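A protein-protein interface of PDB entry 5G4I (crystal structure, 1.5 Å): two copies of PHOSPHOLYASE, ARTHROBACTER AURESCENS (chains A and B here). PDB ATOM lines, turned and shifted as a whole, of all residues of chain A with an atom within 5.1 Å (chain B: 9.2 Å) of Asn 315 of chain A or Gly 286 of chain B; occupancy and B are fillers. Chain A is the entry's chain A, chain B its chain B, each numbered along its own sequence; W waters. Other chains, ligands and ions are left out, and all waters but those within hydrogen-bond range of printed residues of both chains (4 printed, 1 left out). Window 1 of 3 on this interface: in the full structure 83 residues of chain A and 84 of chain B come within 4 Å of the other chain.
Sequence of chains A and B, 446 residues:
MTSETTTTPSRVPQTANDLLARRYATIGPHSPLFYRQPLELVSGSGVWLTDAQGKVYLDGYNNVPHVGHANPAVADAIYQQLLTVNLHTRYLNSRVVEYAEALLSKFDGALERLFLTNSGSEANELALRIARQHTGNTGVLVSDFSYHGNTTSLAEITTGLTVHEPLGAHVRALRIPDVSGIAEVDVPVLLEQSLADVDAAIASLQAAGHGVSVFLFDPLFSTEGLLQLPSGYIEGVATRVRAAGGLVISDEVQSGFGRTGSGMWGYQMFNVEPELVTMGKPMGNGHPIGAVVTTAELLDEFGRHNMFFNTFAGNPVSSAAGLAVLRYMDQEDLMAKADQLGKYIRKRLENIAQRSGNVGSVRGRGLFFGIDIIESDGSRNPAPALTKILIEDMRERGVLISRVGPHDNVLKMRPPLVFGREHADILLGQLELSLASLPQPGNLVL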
ATOM      1  N   ASN A  86      30.733 -23.853  -0.760  1.00  0.00           N
ATOM      2  CA  ASN A  86      30.051 -22.952   0.228  1.00  0.00           C
ATOM      3  C   ASN A  86      28.572 -22.758  -0.026  1.00  0.00           C
ATOM      4  O   ASN A  86      28.100 -21.581  -0.078  1.00  0.00           O
ATOM      5  CB  ASN A  86      30.809 -21.642   0.357  1.00  0.00           C
ATOM      6  CG  ASN A  86      30.347 -20.785   1.560  1.00  0.00           C
ATOM      7  OD1 ASN A  86      29.876 -21.383   2.553  1.00  0.00           O
ATOM      8  ND2 ASN A  86      30.628 -19.489   1.537  1.00  0.00           N
ATOM      9  N   LEU A  87      27.821 -23.862  -0.109  1.00  0.00           N
ATOM     10  CA  LEU A  87      26.394 -23.755  -0.542  1.00  0.00           C
ATOM     11  C   LEU A  87      25.418 -23.907   0.651  1.00  0.00           C
ATOM     12  O   LEU A  87      25.708 -24.520   1.692  1.00  0.00           O
ATOM     13  CB  LEU A  87      26.041 -24.850  -1.579  1.00  0.00           C
ATOM     14  CG  LEU A  87      26.511 -24.566  -3.030  1.00  0.00           C
ATOM     15  CD1 LEU A  87      26.369 -25.803  -3.882  1.00  0.00           C
ATOM     16  CD2 LEU A  87      25.732 -23.382  -3.619  1.00  0.00           C
ATOM     17  N   HIS A  88      24.251 -23.346   0.456  1.00  0.00           N
ATOM     18  CA  HIS A  88      23.119 -23.441   1.402  1.00  0.00           C
ATOM     19  C   HIS A  88      22.706 -24.916   1.677  1.00  0.00           C
ATOM     20  O   HIS A  88      23.088 -25.861   0.944  1.00  0.00           O
ATOM     21  CB  HIS A  88      21.923 -22.643   0.842  1.00  0.00           C
ATOM     22  CG  HIS A  88      21.545 -23.103  -0.545  1.00  0.00           C
ATOM     23  ND1 HIS A  88      20.769 -24.213  -0.758  1.00  0.00           N
ATOM     24  CD2 HIS A  88      21.984 -22.701  -1.777  1.00  0.00           C
ATOM     25  CE1 HIS A  88      20.741 -24.477  -2.067  1.00  0.00           C
ATOM     26  NE2 HIS A  88      21.497 -23.595  -2.705  1.00  0.00           N
ATOM     27  N   THR A  89      21.859 -25.036   2.678  1.00  0.00           N
ATOM     28  CA  THR A  89      21.508 -26.367   3.226  1.00  0.00           C
ATOM     29  C   THR A  89      20.448 -27.140   2.451  1.00  0.00           C
ATOM     30  O   THR A  89      20.065 -28.267   2.946  1.00  0.00           O
ATOM     31  CB  THR A  89      21.025 -26.190   4.667  1.00  0.00           C
ATOM     32  OG1 THR A  89      19.886 -25.260   4.740  1.00  0.00           O
ATOM     33  CG2 THR A  89      22.189 -25.693   5.576  1.00  0.00           C
ATOM     34  N   HIS A 287      32.977 -14.123  12.746  1.00  0.00           N
ATOM     35  CA  HIS A 287      32.148 -14.566  11.578  1.00  0.00           C
ATOM     36  C   HIS A 287      30.672 -14.335  11.933  1.00  0.00           C
ATOM     37  O   HIS A 287      30.252 -14.593  13.114  1.00  0.00           O
ATOM     38  CB  HIS A 287      32.387 -16.033  11.296  1.00  0.00           C
ATOM     39  CG  HIS A 287      31.964 -16.447   9.905  1.00  0.00           C
ATOM     40  ND1 HIS A 287      32.728 -16.167   8.764  1.00  0.00           N
ATOM     41  CD2 HIS A 287      30.833 -17.035   9.433  1.00  0.00           C
ATOM     42  CE1 HIS A 287      32.087 -16.573   7.690  1.00  0.00           C
ATOM     43  NE2 HIS A 287      30.947 -17.141   8.068  1.00  0.00           N
ATOM     44  N   PHE A 312      21.797 -18.055   4.272  1.00  0.00           N
ATOM     45  CA  PHE A 312      23.213 -18.137   4.679  1.00  0.00           C
ATOM     46  C   PHE A 312      23.413 -19.038   5.926  1.00  0.00           C
ATOM     47  O   PHE A 312      24.523 -19.514   6.140  1.00  0.00           O
ATOM     48  CB  PHE A 312      23.791 -16.728   4.984  1.00  0.00           C
ATOM     49  CG  PHE A 312      23.800 -15.765   3.795  1.00  0.00           C
ATOM     50  CD1 PHE A 312      24.318 -16.142   2.570  1.00  0.00           C
ATOM     51  CD2 PHE A 312      23.422 -14.450   4.008  1.00  0.00           C
ATOM     52  CE1 PHE A 312      24.395 -15.195   1.534  1.00  0.00           C
ATOM     53  CE2 PHE A 312      23.500 -13.509   2.982  1.00  0.00           C
ATOM     54  CZ  PHE A 312      23.993 -13.899   1.724  1.00  0.00           C
ATOM     55  N   ALA A 313      22.336 -19.332   6.673  1.00  0.00           N
ATOM     56  CA  ALA A 313      22.539 -20.079   7.910  1.00  0.00           C
ATOM     57  C   ALA A 313      23.045 -21.484   7.663  1.00  0.00           C
ATOM     58  O   ALA A 313      22.520 -22.191   6.737  1.00  0.00           O
ATOM     59  CB  ALA A 313      21.252 -20.153   8.693  1.00  0.00           C
ATOM     60  N   GLY A 314      24.048 -21.932   8.443  1.00  0.00           N
ATOM     61  CA  GLY A 314      24.502 -23.327   8.237  1.00  0.00           C
ATOM     62  C   GLY A 314      25.254 -23.619   6.990  1.00  0.00           C
ATOM     63  O   GLY A 314      25.386 -24.797   6.584  1.00  0.00           O
ATOM     64  N   ASN A 315      25.675 -22.587   6.274  1.00  0.00           N
ATOM     65  CA  ASN A 315      26.570 -22.842   5.158  1.00  0.00           C
ATOM     66  C   ASN A 315      27.878 -23.498   5.678  1.00  0.00           C
ATOM     67  O   ASN A 315      28.212 -23.401   6.865  1.00  0.00           O
ATOM     68  CB  ASN A 315      26.823 -21.523   4.367  1.00  0.00           C
ATOM     69  CG  ASN A 315      27.767 -20.532   5.084  1.00  0.00           C
ATOM     70  OD1 ASN A 315      28.966 -20.755   5.221  1.00  0.00           O
ATOM     71  ND2 ASN A 315      27.221 -19.421   5.556  1.00  0.00           N
ATOM     72  N   PRO A 316      28.670 -24.206   4.804  1.00  0.00           N
ATOM     73  CA  PRO A 316      29.792 -24.930   5.264  1.00  0.00           C
ATOM     74  C   PRO A 316      30.940 -24.070   5.891  1.00  0.00           C
ATOM     75  O   PRO A 316      31.674 -24.548   6.748  1.00  0.00           O
ATOM     76  CB  PRO A 316      30.334 -25.623   3.967  1.00  0.00           C
ATOM     77  CG  PRO A 316      29.157 -25.674   3.047  1.00  0.00           C
ATOM     78  CD  PRO A 316      28.365 -24.457   3.374  1.00  0.00           C
ATOM     79  N   VAL A 317      31.101 -22.818   5.380  1.00  0.00           N
ATOM     80  CA  VAL A 317      32.155 -21.928   5.867  1.00  0.00           C
ATOM     81  C   VAL A 317      31.869 -21.372   7.309  1.00  0.00           C
ATOM     82  O   VAL A 317      32.697 -21.436   8.223  1.00  0.00           O
ATOM     83  CB  VAL A 317      32.448 -20.811   4.854  1.00  0.00           C
ATOM     84  CG1 VAL A 317      33.399 -19.801   5.454  1.00  0.00           C
ATOM     85  CG2 VAL A 317      33.033 -21.431   3.603  1.00  0.00           C
ATOM     86  N   SER A 318      30.614 -20.920   7.527  1.00  0.00           N
ATOM     87  CA  SER A 318      30.135 -20.612   8.873  1.00  0.00           C
ATOM     88  C   SER A 318      30.274 -21.816   9.831  1.00  0.00           C
ATOM     89  O   SER A 318      30.734 -21.636  10.970  1.00  0.00           O
ATOM     90  CB  SER A 318      28.657 -20.161   8.826  1.00  0.00           C
ATOM     91  OG  SER A 318      28.531 -18.885   8.183  1.00  0.00           O
ATOM     92  N   SER A 319      29.913 -23.001   9.344  1.00  0.00           N
ATOM     93  CA  SER A 319      30.039 -24.225  10.166  1.00  0.00           C
ATOM     94  C   SER A 319      31.501 -24.494  10.509  1.00  0.00           C
ATOM     95  O   SER A 319      31.810 -24.880  11.659  1.00  0.00           O
ATOM     96  CB  SER A 319      29.400 -25.392   9.429  1.00  0.00           C
ATOM     97  OG  SER A 319      27.995 -25.163   9.146  1.00  0.00           O
ATOM     98  N   ALA A 320      32.415 -24.350   9.542  1.00  0.00           N
ATOM     99  CA  ALA A 320      33.883 -24.531   9.779  1.00  0.00           C
ATOM    100  C   ALA A 320      34.377 -23.552  10.851  1.00  0.00           C
ATOM    101  O   ALA A 320      35.176 -23.898  11.749  1.00  0.00           O
ATOM    102  CB  ALA A 320      34.661 -24.434   8.459  1.00  0.00           C
ATOM    103  N   ILE B  27      19.241 -30.692  12.984  1.00  0.00           N
ATOM    104  CA  ILE B  27      18.508 -29.550  12.394  1.00  0.00           C
ATOM    105  C   ILE B  27      17.087 -29.928  11.946  1.00  0.00           C
ATOM    106  O   ILE B  27      16.306 -29.063  11.578  1.00  0.00           O
ATOM    107  CB  ILE B  27      19.316 -28.835  11.353  1.00  0.00           C
ATOM    108  CG1 ILE B  27      19.636 -29.701  10.186  1.00  0.00           C
ATOM    109  CG2 ILE B  27      20.620 -28.238  11.898  1.00  0.00           C
ATOM    110  CD1 ILE B  27      20.196 -28.931   8.944  1.00  0.00           C
ATOM    111  N   ASN B  63      22.644 -18.632  -7.295  1.00  0.00           N
ATOM    112  CA  ASN B  63      23.042 -17.217  -7.379  1.00  0.00           C
ATOM    113  C   ASN B  63      23.908 -16.701  -6.211  1.00  0.00           C
ATOM    114  O   ASN B  63      24.572 -15.648  -6.348  1.00  0.00           O
ATOM    115  CB  ASN B  63      21.813 -16.288  -7.521  1.00  0.00           C
ATOM    116  CG  ASN B  63      20.864 -16.357  -6.345  1.00  0.00           C
ATOM    117  OD1 ASN B  63      20.877 -17.253  -5.533  1.00  0.00           O
ATOM    118  ND2 ASN B  63      19.995 -15.295  -6.272  1.00  0.00           N
ATOM    119  N   VAL B  64      23.969 -17.436  -5.110  1.00  0.00           N
ATOM    120  CA  VAL B  64      24.850 -16.969  -4.009  1.00  0.00           C
ATOM    121  C   VAL B  64      26.347 -16.933  -4.409  1.00  0.00           C
ATOM    122  O   VAL B  64      27.065 -15.963  -4.115  1.00  0.00           O
ATOM    123  CB  VAL B  64      24.584 -17.831  -2.716  1.00  0.00           C
ATOM    124  CG1 VAL B  64      25.657 -17.620  -1.666  1.00  0.00           C
ATOM    125  CG2 VAL B  64      23.189 -17.502  -2.189  1.00  0.00           C
ATOM    126  N   PRO B  65      26.901 -18.014  -5.065  1.00  0.00           N
ATOM    127  CA  PRO B  65      28.274 -17.962  -5.598  1.00  0.00           C
ATOM    128  C   PRO B  65      28.331 -17.117  -6.884  1.00  0.00           C
ATOM    129  O   PRO B  65      28.669 -17.656  -8.019  1.00  0.00           O
ATOM    130  CB  PRO B  65      28.615 -19.453  -5.876  1.00  0.00           C
ATOM    131  CG  PRO B  65      27.305 -20.037  -6.170  1.00  0.00           C
ATOM    132  CD  PRO B  65      26.288 -19.338  -5.294  1.00  0.00           C
ATOM    133  N   HIS B  66      28.057 -15.834  -6.757  1.00  0.00           N
ATOM    134  CA  HIS B  66      27.965 -14.876  -7.883  1.00  0.00           C
ATOM    135  C   HIS B  66      29.194 -14.928  -8.811  1.00  0.00           C
ATOM    136  O   HIS B  66      29.024 -14.837 -10.058  1.00  0.00           O
ATOM    137  CB  HIS B  66      27.888 -13.473  -7.267  1.00  0.00           C
ATOM    138  CG  HIS B  66      27.520 -12.376  -8.224  1.00  0.00           C
ATOM    139  ND1 HIS B  66      26.330 -12.379  -8.905  1.00  0.00           N
ATOM    140  CD2 HIS B  66      28.199 -11.280  -8.623  1.00  0.00           C
ATOM    141  CE1 HIS B  66      26.259 -11.284  -9.658  1.00  0.00           C
ATOM    142  NE2 HIS B  66      27.384 -10.610  -9.516  1.00  0.00           N
ATOM    143  N   VAL B  67      30.384 -14.988  -8.244  1.00  0.00           N
ATOM    144  CA  VAL B  67      31.638 -14.988  -9.004  1.00  0.00           C
ATOM    145  C   VAL B  67      32.303 -16.385  -9.070  1.00  0.00           C
ATOM    146  O   VAL B  67      33.509 -16.507  -9.377  1.00  0.00           O
ATOM    147  CB  VAL B  67      32.634 -13.873  -8.578  1.00  0.00           C
ATOM    148  CG1 VAL B  67      32.021 -12.503  -8.864  1.00  0.00           C
ATOM    149  CG2 VAL B  67      32.987 -13.986  -7.120  1.00  0.00           C
ATOM    150  N   GLY B  68      31.514 -17.417  -8.806  1.00  0.00           N
ATOM    151  CA  GLY B  68      31.874 -18.839  -8.993  1.00  0.00           C
ATOM    152  C   GLY B  68      32.259 -19.580  -7.733  1.00  0.00           C
ATOM    153  O   GLY B  68      32.768 -18.943  -6.754  1.00  0.00           O
ATOM    154  N   HIS B  69      31.972 -20.894  -7.666  1.00  0.00           N
ATOM    155  CA  HIS B  69      32.369 -21.748  -6.555  1.00  0.00           C
ATOM    156  C   HIS B  69      33.877 -21.651  -6.308  1.00  0.00           C
ATOM    157  O   HIS B  69      34.707 -21.733  -7.279  1.00  0.00           O
ATOM    158  CB  HIS B  69      31.929 -23.190  -6.824  1.00  0.00           C
ATOM    159  CG  HIS B  69      30.445 -23.317  -6.986  1.00  0.00           C
ATOM    160  ND1 HIS B  69      29.565 -23.258  -5.910  1.00  0.00           N
ATOM    161  CD2 HIS B  69      29.682 -23.580  -8.059  1.00  0.00           C
ATOM    162  CE1 HIS B  69      28.334 -23.438  -6.339  1.00  0.00           C
ATOM    163  NE2 HIS B  69      28.363 -23.652  -7.639  1.00  0.00           N
ATOM    164  N   ALA B  70      34.280 -21.530  -5.025  1.00  0.00           N
ATOM    165  CA  ALA B  70      35.688 -21.522  -4.607  1.00  0.00           C
ATOM    166  C   ALA B  70      36.481 -20.398  -5.226  1.00  0.00           C
ATOM    167  O   ALA B  70      37.739 -20.512  -5.332  1.00  0.00           O
ATOM    168  CB  ALA B  70      36.272 -22.873  -4.835  1.00  0.00           C
ATOM    169  N   ASN B  71      35.853 -19.285  -5.605  1.00  0.00           N
ATOM    170  CA  ASN B  71      36.607 -18.164  -6.200  1.00  0.00           C
ATOM    171  C   ASN B  71      37.811 -17.791  -5.305  1.00  0.00           C
ATOM    172  O   ASN B  71      37.664 -17.494  -4.089  1.00  0.00           O
ATOM    173  CB  ASN B  71      35.695 -16.937  -6.397  1.00  0.00           C
ATOM    174  CG  ASN B  71      36.418 -15.750  -7.026  1.00  0.00           C
ATOM    175  OD1 ASN B  71      37.393 -15.212  -6.440  1.00  0.00           O
ATOM    176  ND2 ASN B  71      36.000 -15.381  -8.228  1.00  0.00           N
ATOM    177  N   VAL B  74      38.159 -14.025  -3.767  1.00  0.00           N
ATOM    178  CA  VAL B  74      37.301 -13.833  -2.577  1.00  0.00           C
ATOM    179  C   VAL B  74      37.924 -14.562  -1.372  1.00  0.00           C
ATOM    180  O   VAL B  74      38.009 -14.010  -0.248  1.00  0.00           O
ATOM    181  CB  VAL B  74      35.857 -14.258  -2.829  1.00  0.00           C
ATOM    182  CG1 VAL B  74      35.004 -14.083  -1.515  1.00  0.00           C
ATOM    183  CG2 VAL B  74      35.252 -13.467  -3.965  1.00  0.00           C
ATOM    184  N   ILE B  78      39.355 -12.666   2.220  1.00  0.00           N
ATOM    185  CA  ILE B  78      38.884 -13.075   3.564  1.00  0.00           C
ATOM    186  C   ILE B  78      39.995 -13.505   4.486  1.00  0.00           C
ATOM    187  O   ILE B  78      40.130 -13.055   5.629  1.00  0.00           O
ATOM    188  CB  ILE B  78      37.712 -14.084   3.397  1.00  0.00           C
ATOM    189  CG1 ILE B  78      36.447 -13.431   2.787  1.00  0.00           C
ATOM    190  CG2 ILE B  78      37.446 -14.788   4.681  1.00  0.00           C
ATOM    191  CD1 ILE B  78      35.315 -14.436   2.302  1.00  0.00           C
ATOM    192  N   ASN B 118      23.661  -8.602   7.861  1.00  0.00           N
ATOM    193  CA  ASN B 118      24.263  -9.913   7.585  1.00  0.00           C
ATOM    194  C   ASN B 118      23.380 -10.879   6.731  1.00  0.00           C
ATOM    195  O   ASN B 118      23.766 -12.038   6.555  1.00  0.00           O
ATOM    196  CB  ASN B 118      24.591 -10.608   8.933  1.00  0.00           C
ATOM    197  CG  ASN B 118      25.300  -9.703   9.938  1.00  0.00           C
ATOM    198  OD1 ASN B 118      24.671  -9.234  10.941  1.00  0.00           O
ATOM    199  ND2 ASN B 118      26.499  -9.341   9.680  1.00  0.00           N
ATOM    200  N   GLY B 280      21.249  -8.848  -0.733  1.00  0.00           N
ATOM    201  CA  GLY B 280      21.756  -9.997   0.031  1.00  0.00           C
ATOM    202  C   GLY B 280      22.406 -11.018  -0.946  1.00  0.00           C
ATOM    203  O   GLY B 280      23.157 -10.632  -1.893  1.00  0.00           O
ATOM    204  N   LYS B 281      21.941 -12.274  -0.845  1.00  0.00           N
ATOM    205  CA  LYS B 281      22.437 -13.460  -1.600  1.00  0.00           C
ATOM    206  C   LYS B 281      23.813 -13.358  -2.292  1.00  0.00           C
ATOM    207  O   LYS B 281      24.785 -13.734  -1.637  1.00  0.00           O
ATOM    208  CB  LYS B 281      21.278 -14.109  -2.468  1.00  0.00           C
ATOM    209  CG  LYS B 281      20.199 -14.847  -1.606  1.00  0.00           C
ATOM    210  CD  LYS B 281      19.223 -15.584  -2.500  1.00  0.00           C
ATOM    211  CE  LYS B 281      18.142 -16.447  -1.776  1.00  0.00           C
ATOM    212  NZ  LYS B 281      16.871 -15.611  -1.573  1.00  0.00           N
ATOM    213  N   PRO B 282      23.899 -12.922  -3.576  1.00  0.00           N
ATOM    214  CA  PRO B 282      25.235 -12.822  -4.149  1.00  0.00           C
ATOM    215  C   PRO B 282      26.363 -11.994  -3.499  1.00  0.00           C
ATOM    216  O   PRO B 282      27.559 -12.121  -3.900  1.00  0.00           O
ATOM    217  CB  PRO B 282      24.930 -12.213  -5.542  1.00  0.00           C
ATOM    218  CG  PRO B 282      23.732 -11.364  -5.348  1.00  0.00           C
ATOM    219  CD  PRO B 282      22.921 -12.287  -4.466  1.00  0.00           C
ATOM    220  N   MET B 283      26.028 -11.015  -2.655  1.00  0.00           N
ATOM    221  CA  MET B 283      26.897  -9.878  -2.355  1.00  0.00           C
ATOM    222  C   MET B 283      28.296 -10.195  -1.876  1.00  0.00           C
ATOM    223  O   MET B 283      29.269  -9.482  -2.112  1.00  0.00           O
ATOM    224  CB  MET B 283      26.061  -9.116  -1.283  1.00  0.00           C
ATOM    225  CG  MET B 283      26.576  -7.931  -0.704  1.00  0.00           C
ATOM    226  SD  MET B 283      25.170  -7.190   0.243  1.00  0.00           S
ATOM    227  CE  MET B 283      26.056  -5.781   0.344  1.00  0.00           C
ATOM    228  N   GLY B 284      28.406 -11.297  -1.091  1.00  0.00           N
ATOM    229  CA  GLY B 284      29.678 -11.822  -0.591  1.00  0.00           C
ATOM    230  C   GLY B 284      30.134 -13.210  -1.055  1.00  0.00           C
ATOM    231  O   GLY B 284      30.949 -13.858  -0.407  1.00  0.00           O
ATOM    232  N   ASN B 285      29.547 -13.628  -2.213  1.00  0.00           N
ATOM    233  CA  ASN B 285      29.830 -14.956  -2.813  1.00  0.00           C
ATOM    234  C   ASN B 285      29.488 -16.119  -1.899  1.00  0.00           C
ATOM    235  O   ASN B 285      29.905 -17.232  -2.145  1.00  0.00           O
ATOM    236  CB  ASN B 285      31.300 -15.141  -3.222  1.00  0.00           C
ATOM    237  CG  ASN B 285      31.452 -15.986  -4.455  1.00  0.00           C
ATOM    238  OD1 ASN B 285      30.692 -15.811  -5.443  1.00  0.00           O
ATOM    239  ND2 ASN B 285      32.438 -16.903  -4.446  1.00  0.00           N
ATOM    240  N   GLY B 286      28.669 -15.861  -0.881  1.00  0.00           N
ATOM    241  CA  GLY B 286      28.348 -16.871   0.135  1.00  0.00           C
ATOM    242  C   GLY B 286      28.648 -16.469   1.581  1.00  0.00           C
ATOM    243  O   GLY B 286      28.233 -17.147   2.549  1.00  0.00           O
ATOM    244  N   HIS B 287      29.411 -15.416   1.792  1.00  0.00           N
ATOM    245  CA  HIS B 287      29.604 -14.806   3.109  1.00  0.00           C
ATOM    246  C   HIS B 287      28.267 -14.138   3.531  1.00  0.00           C
ATOM    247  O   HIS B 287      27.575 -13.551   2.701  1.00  0.00           O
ATOM    248  CB  HIS B 287      30.704 -13.696   3.040  1.00  0.00           C
ATOM    249  CG  HIS B 287      31.371 -13.430   4.364  1.00  0.00           C
ATOM    250  ND1 HIS B 287      31.129 -12.370   5.266  1.00  0.00           N
ATOM    251  CD2 HIS B 287      32.293 -14.197   4.962  1.00  0.00           C
ATOM    252  CE1 HIS B 287      31.908 -12.527   6.335  1.00  0.00           C
ATOM    253  NE2 HIS B 287      32.569 -13.639   6.177  1.00  0.00           N
ATOM    254  N   PRO B 288      27.941 -14.181   4.839  1.00  0.00           N
ATOM    255  CA  PRO B 288      26.654 -13.569   5.210  1.00  0.00           C
ATOM    256  C   PRO B 288      26.780 -12.016   5.249  1.00  0.00           C
ATOM    257  O   PRO B 288      27.312 -11.450   6.164  1.00  0.00           O
ATOM    258  CB  PRO B 288      26.387 -14.164   6.594  1.00  0.00           C
ATOM    259  CG  PRO B 288      27.326 -15.345   6.771  1.00  0.00           C
ATOM    260  CD  PRO B 288      28.557 -14.860   6.002  1.00  0.00           C
ATOM    261  N   ILE B 289      26.196 -11.394   4.211  1.00  0.00           N
ATOM    262  CA  ILE B 289      26.183  -9.945   4.052  1.00  0.00           C
ATOM    263  C   ILE B 289      24.838  -9.539   3.419  1.00  0.00           C
ATOM    264  O   ILE B 289      24.303 -10.220   2.502  1.00  0.00           O
ATOM    265  CB  ILE B 289      27.343  -9.403   3.155  1.00  0.00           C
ATOM    266  CG1 ILE B 289      28.677  -9.984   3.452  1.00  0.00           C
ATOM    267  CG2 ILE B 289      27.380  -7.844   3.265  1.00  0.00           C
ATOM    268  CD1 ILE B 289      29.745  -9.525   2.468  1.00  0.00           C
ATOM    269  N   SER B 318      33.884  -9.239   6.440  1.00  0.00           N
ATOM    270  CA  SER B 318      32.699  -9.059   5.556  1.00  0.00           C
ATOM    271  C   SER B 318      32.903  -7.985   4.495  1.00  0.00           C
ATOM    272  O   SER B 318      32.604  -8.183   3.321  1.00  0.00           O
ATOM    273  CB  SER B 318      31.436  -8.706   6.349  1.00  0.00           C
ATOM    274  OG  SER B 318      30.988  -9.827   7.188  1.00  0.00           O
ATOM    275  N   ALA B 321      35.293  -9.300   1.805  1.00  0.00           N
ATOM    276  CA  ALA B 321      34.579 -10.197   0.887  1.00  0.00           C
ATOM    277  C   ALA B 321      33.758  -9.444  -0.127  1.00  0.00           C
ATOM    278  O   ALA B 321      33.775  -9.755  -1.366  1.00  0.00           O
ATOM    279  CB  ALA B 321      33.653 -11.113   1.701  1.00  0.00           C
ATOM    280  N   GLY B 322      32.966  -8.488   0.332  1.00  0.00           N
ATOM    281  CA  GLY B 322      32.155  -7.668  -0.585  1.00  0.00           C
ATOM    282  C   GLY B 322      32.988  -6.854  -1.569  1.00  0.00           C
ATOM    283  O   GLY B 322      32.596  -6.773  -2.763  1.00  0.00           O
ATOM    284  N   VAL B 325      34.204  -9.294  -4.376  1.00  0.00           N
ATOM    285  CA  VAL B 325      33.153  -9.577  -5.334  1.00  0.00           C
ATOM    286  C   VAL B 325      32.985  -8.433  -6.402  1.00  0.00           C
ATOM    287  O   VAL B 325      32.905  -8.735  -7.630  1.00  0.00           O
ATOM    288  CB  VAL B 325      31.770  -9.874  -4.635  1.00  0.00           C
ATOM    289  CG1 VAL B 325      30.608  -9.945  -5.621  1.00  0.00           C
ATOM    290  CG2 VAL B 325      31.908 -11.186  -3.862  1.00  0.00           C
HETATM  291  O   HOH W   1      26.752 -19.481   1.779  1.00  0.00           O
HETATM  292  O   HOH W   2      28.647 -19.960  -2.402  1.00  0.00           O
HETATM  293  O   HOH W   3      29.971 -22.413  -3.252  1.00  0.00           O
HETATM  294  O   HOH W   4      30.098 -18.012   4.764  1.00  0.00           O
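CE1 of His 69 of chain B touches CD2 of Leu 87 of chain A (3.8 Å).
CE1 of His 287 of chain A touches NE2 of His 287 of chain B, 3.3 Å away.
Pro 288 of chain B touches His 287 of chain A (CD to NE2, 3.9 Å).
O of Asn 118 of chain B touches CD2 of Phe 312 of chain A, at 3.5 Å.
Phe 312 of chain A touches Lys 281 of chain B.
Phe 312 of chain A touches His 287 of chain B.
Pro 288 of chain B touches Phe 312 of chain A (CA to CD2, 3.6 Å).
Ile 289 of chain B touches Phe 312 of chain A.
ND2 of Asn 315 of chain A touches O of Gly 286 of chain B, 3.9 Å away.
Printed residues of chain B within 4 Å of Asn 86 of chain A: Gly 286 (3.5 Å).
Of the printed residues of chain B, His 287 of chain A touches His 287 and Pro 288.
Of the printed residues of chain B, Phe 312 of chain A touches Asn 118, Lys 281, His 287, Pro 288 and Ile 289.
Ala 313 of chain A touches none of the printed residues of chain B.
No residue of chain B comes within 4 Å of Gly 314 of chain A.
Asn 315 of chain A touches just one residue of chain B: Gly 286 (3.9 Å).
No residue of chain B comes within 4 Å of Pro 316 of chain A.
Pro 282 of chain B touches none of the printed residues of chain A.
Of the printed residues of chain A, Gly 286 of chain B touches Asn 86 (3.5 Å) and Asn 315 (3.9 Å).
The nearest residue of chain B that does not touch Asn 315 of chain A is Pro 288 of chain B (4.3 Å).
The nearest residue of chain A that does not touch Gly 286 of chain B is Phe 312 of chain A (4.04 Å).
ND2 of Asn 86 of chain A lies within hydrogen-bond range of O of Gly 286 of chain B (3.5 Å).
His 287 of chain B touches its own counterpart, His 287 of chain A.
2 positions are printed for both chains.
Of the 11 pairs that touch across the chains among the printed residues, 1 has its exchanged pair printed and touching as well.
Hydrophobic or aromatic side chains of chain B that line the printed part of chain A: His 69, His 287 and Pro 288.
Of the 14 printed residues of chain A, 6 touch a printed residue of chain B.
Among the printed residues, 11 pairs touch across the chains.
Among the printed residues, no Asp or Glu carboxylate lies within 4 Å of a Lys or Arg side-chain nitrogen of the other chain.
Water W3 lies within hydrogen-bond range of ND1 of His 69 of chain B (2.8 Å) and N of Asn 86 of chain A (3.0 Å).
Water W1 bridges the backbone carbonyl oxygen of Gly 286 of chain B (2.9 Å) and the backbone carbonyl oxygen of Asn 86 of chain A (3.1 Å).
Water W2 bridges the backbone carbonyl oxygen of Asn 86 of chain A (2.9 Å) and the backbone carbonyl oxygen of Asn 285 of chain B (3.0 Å).
Water W4 bridges the side-chain amide oxygen (OD1) of Asn 315 of chain A and the backbone carbonyl oxygen (O) of Gly 286 of chain B.
The side-chain amide oxygen of Asn 86 of chain A sits close to the backbone NH of Val 317 of chain A (3.4 Å).
The side-chain amide nitrogen of Asn 315 of chain A sits at hydrogen-bond distance from the backbone carbonyl oxygen of Phe 312 of chain A.
The side-chain amide oxygen (OD1) of Asn 315 of chain A sits at hydrogen-bond distance from the backbone NH (N) of Val 317 of chain A, 3.0 Å away.
The side-chain amide oxygen (OD1) of Asn 315 of chain A lies within hydrogen-bond range of the backbone NH (N) of Ser 318 of chain A (2.8 Å).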
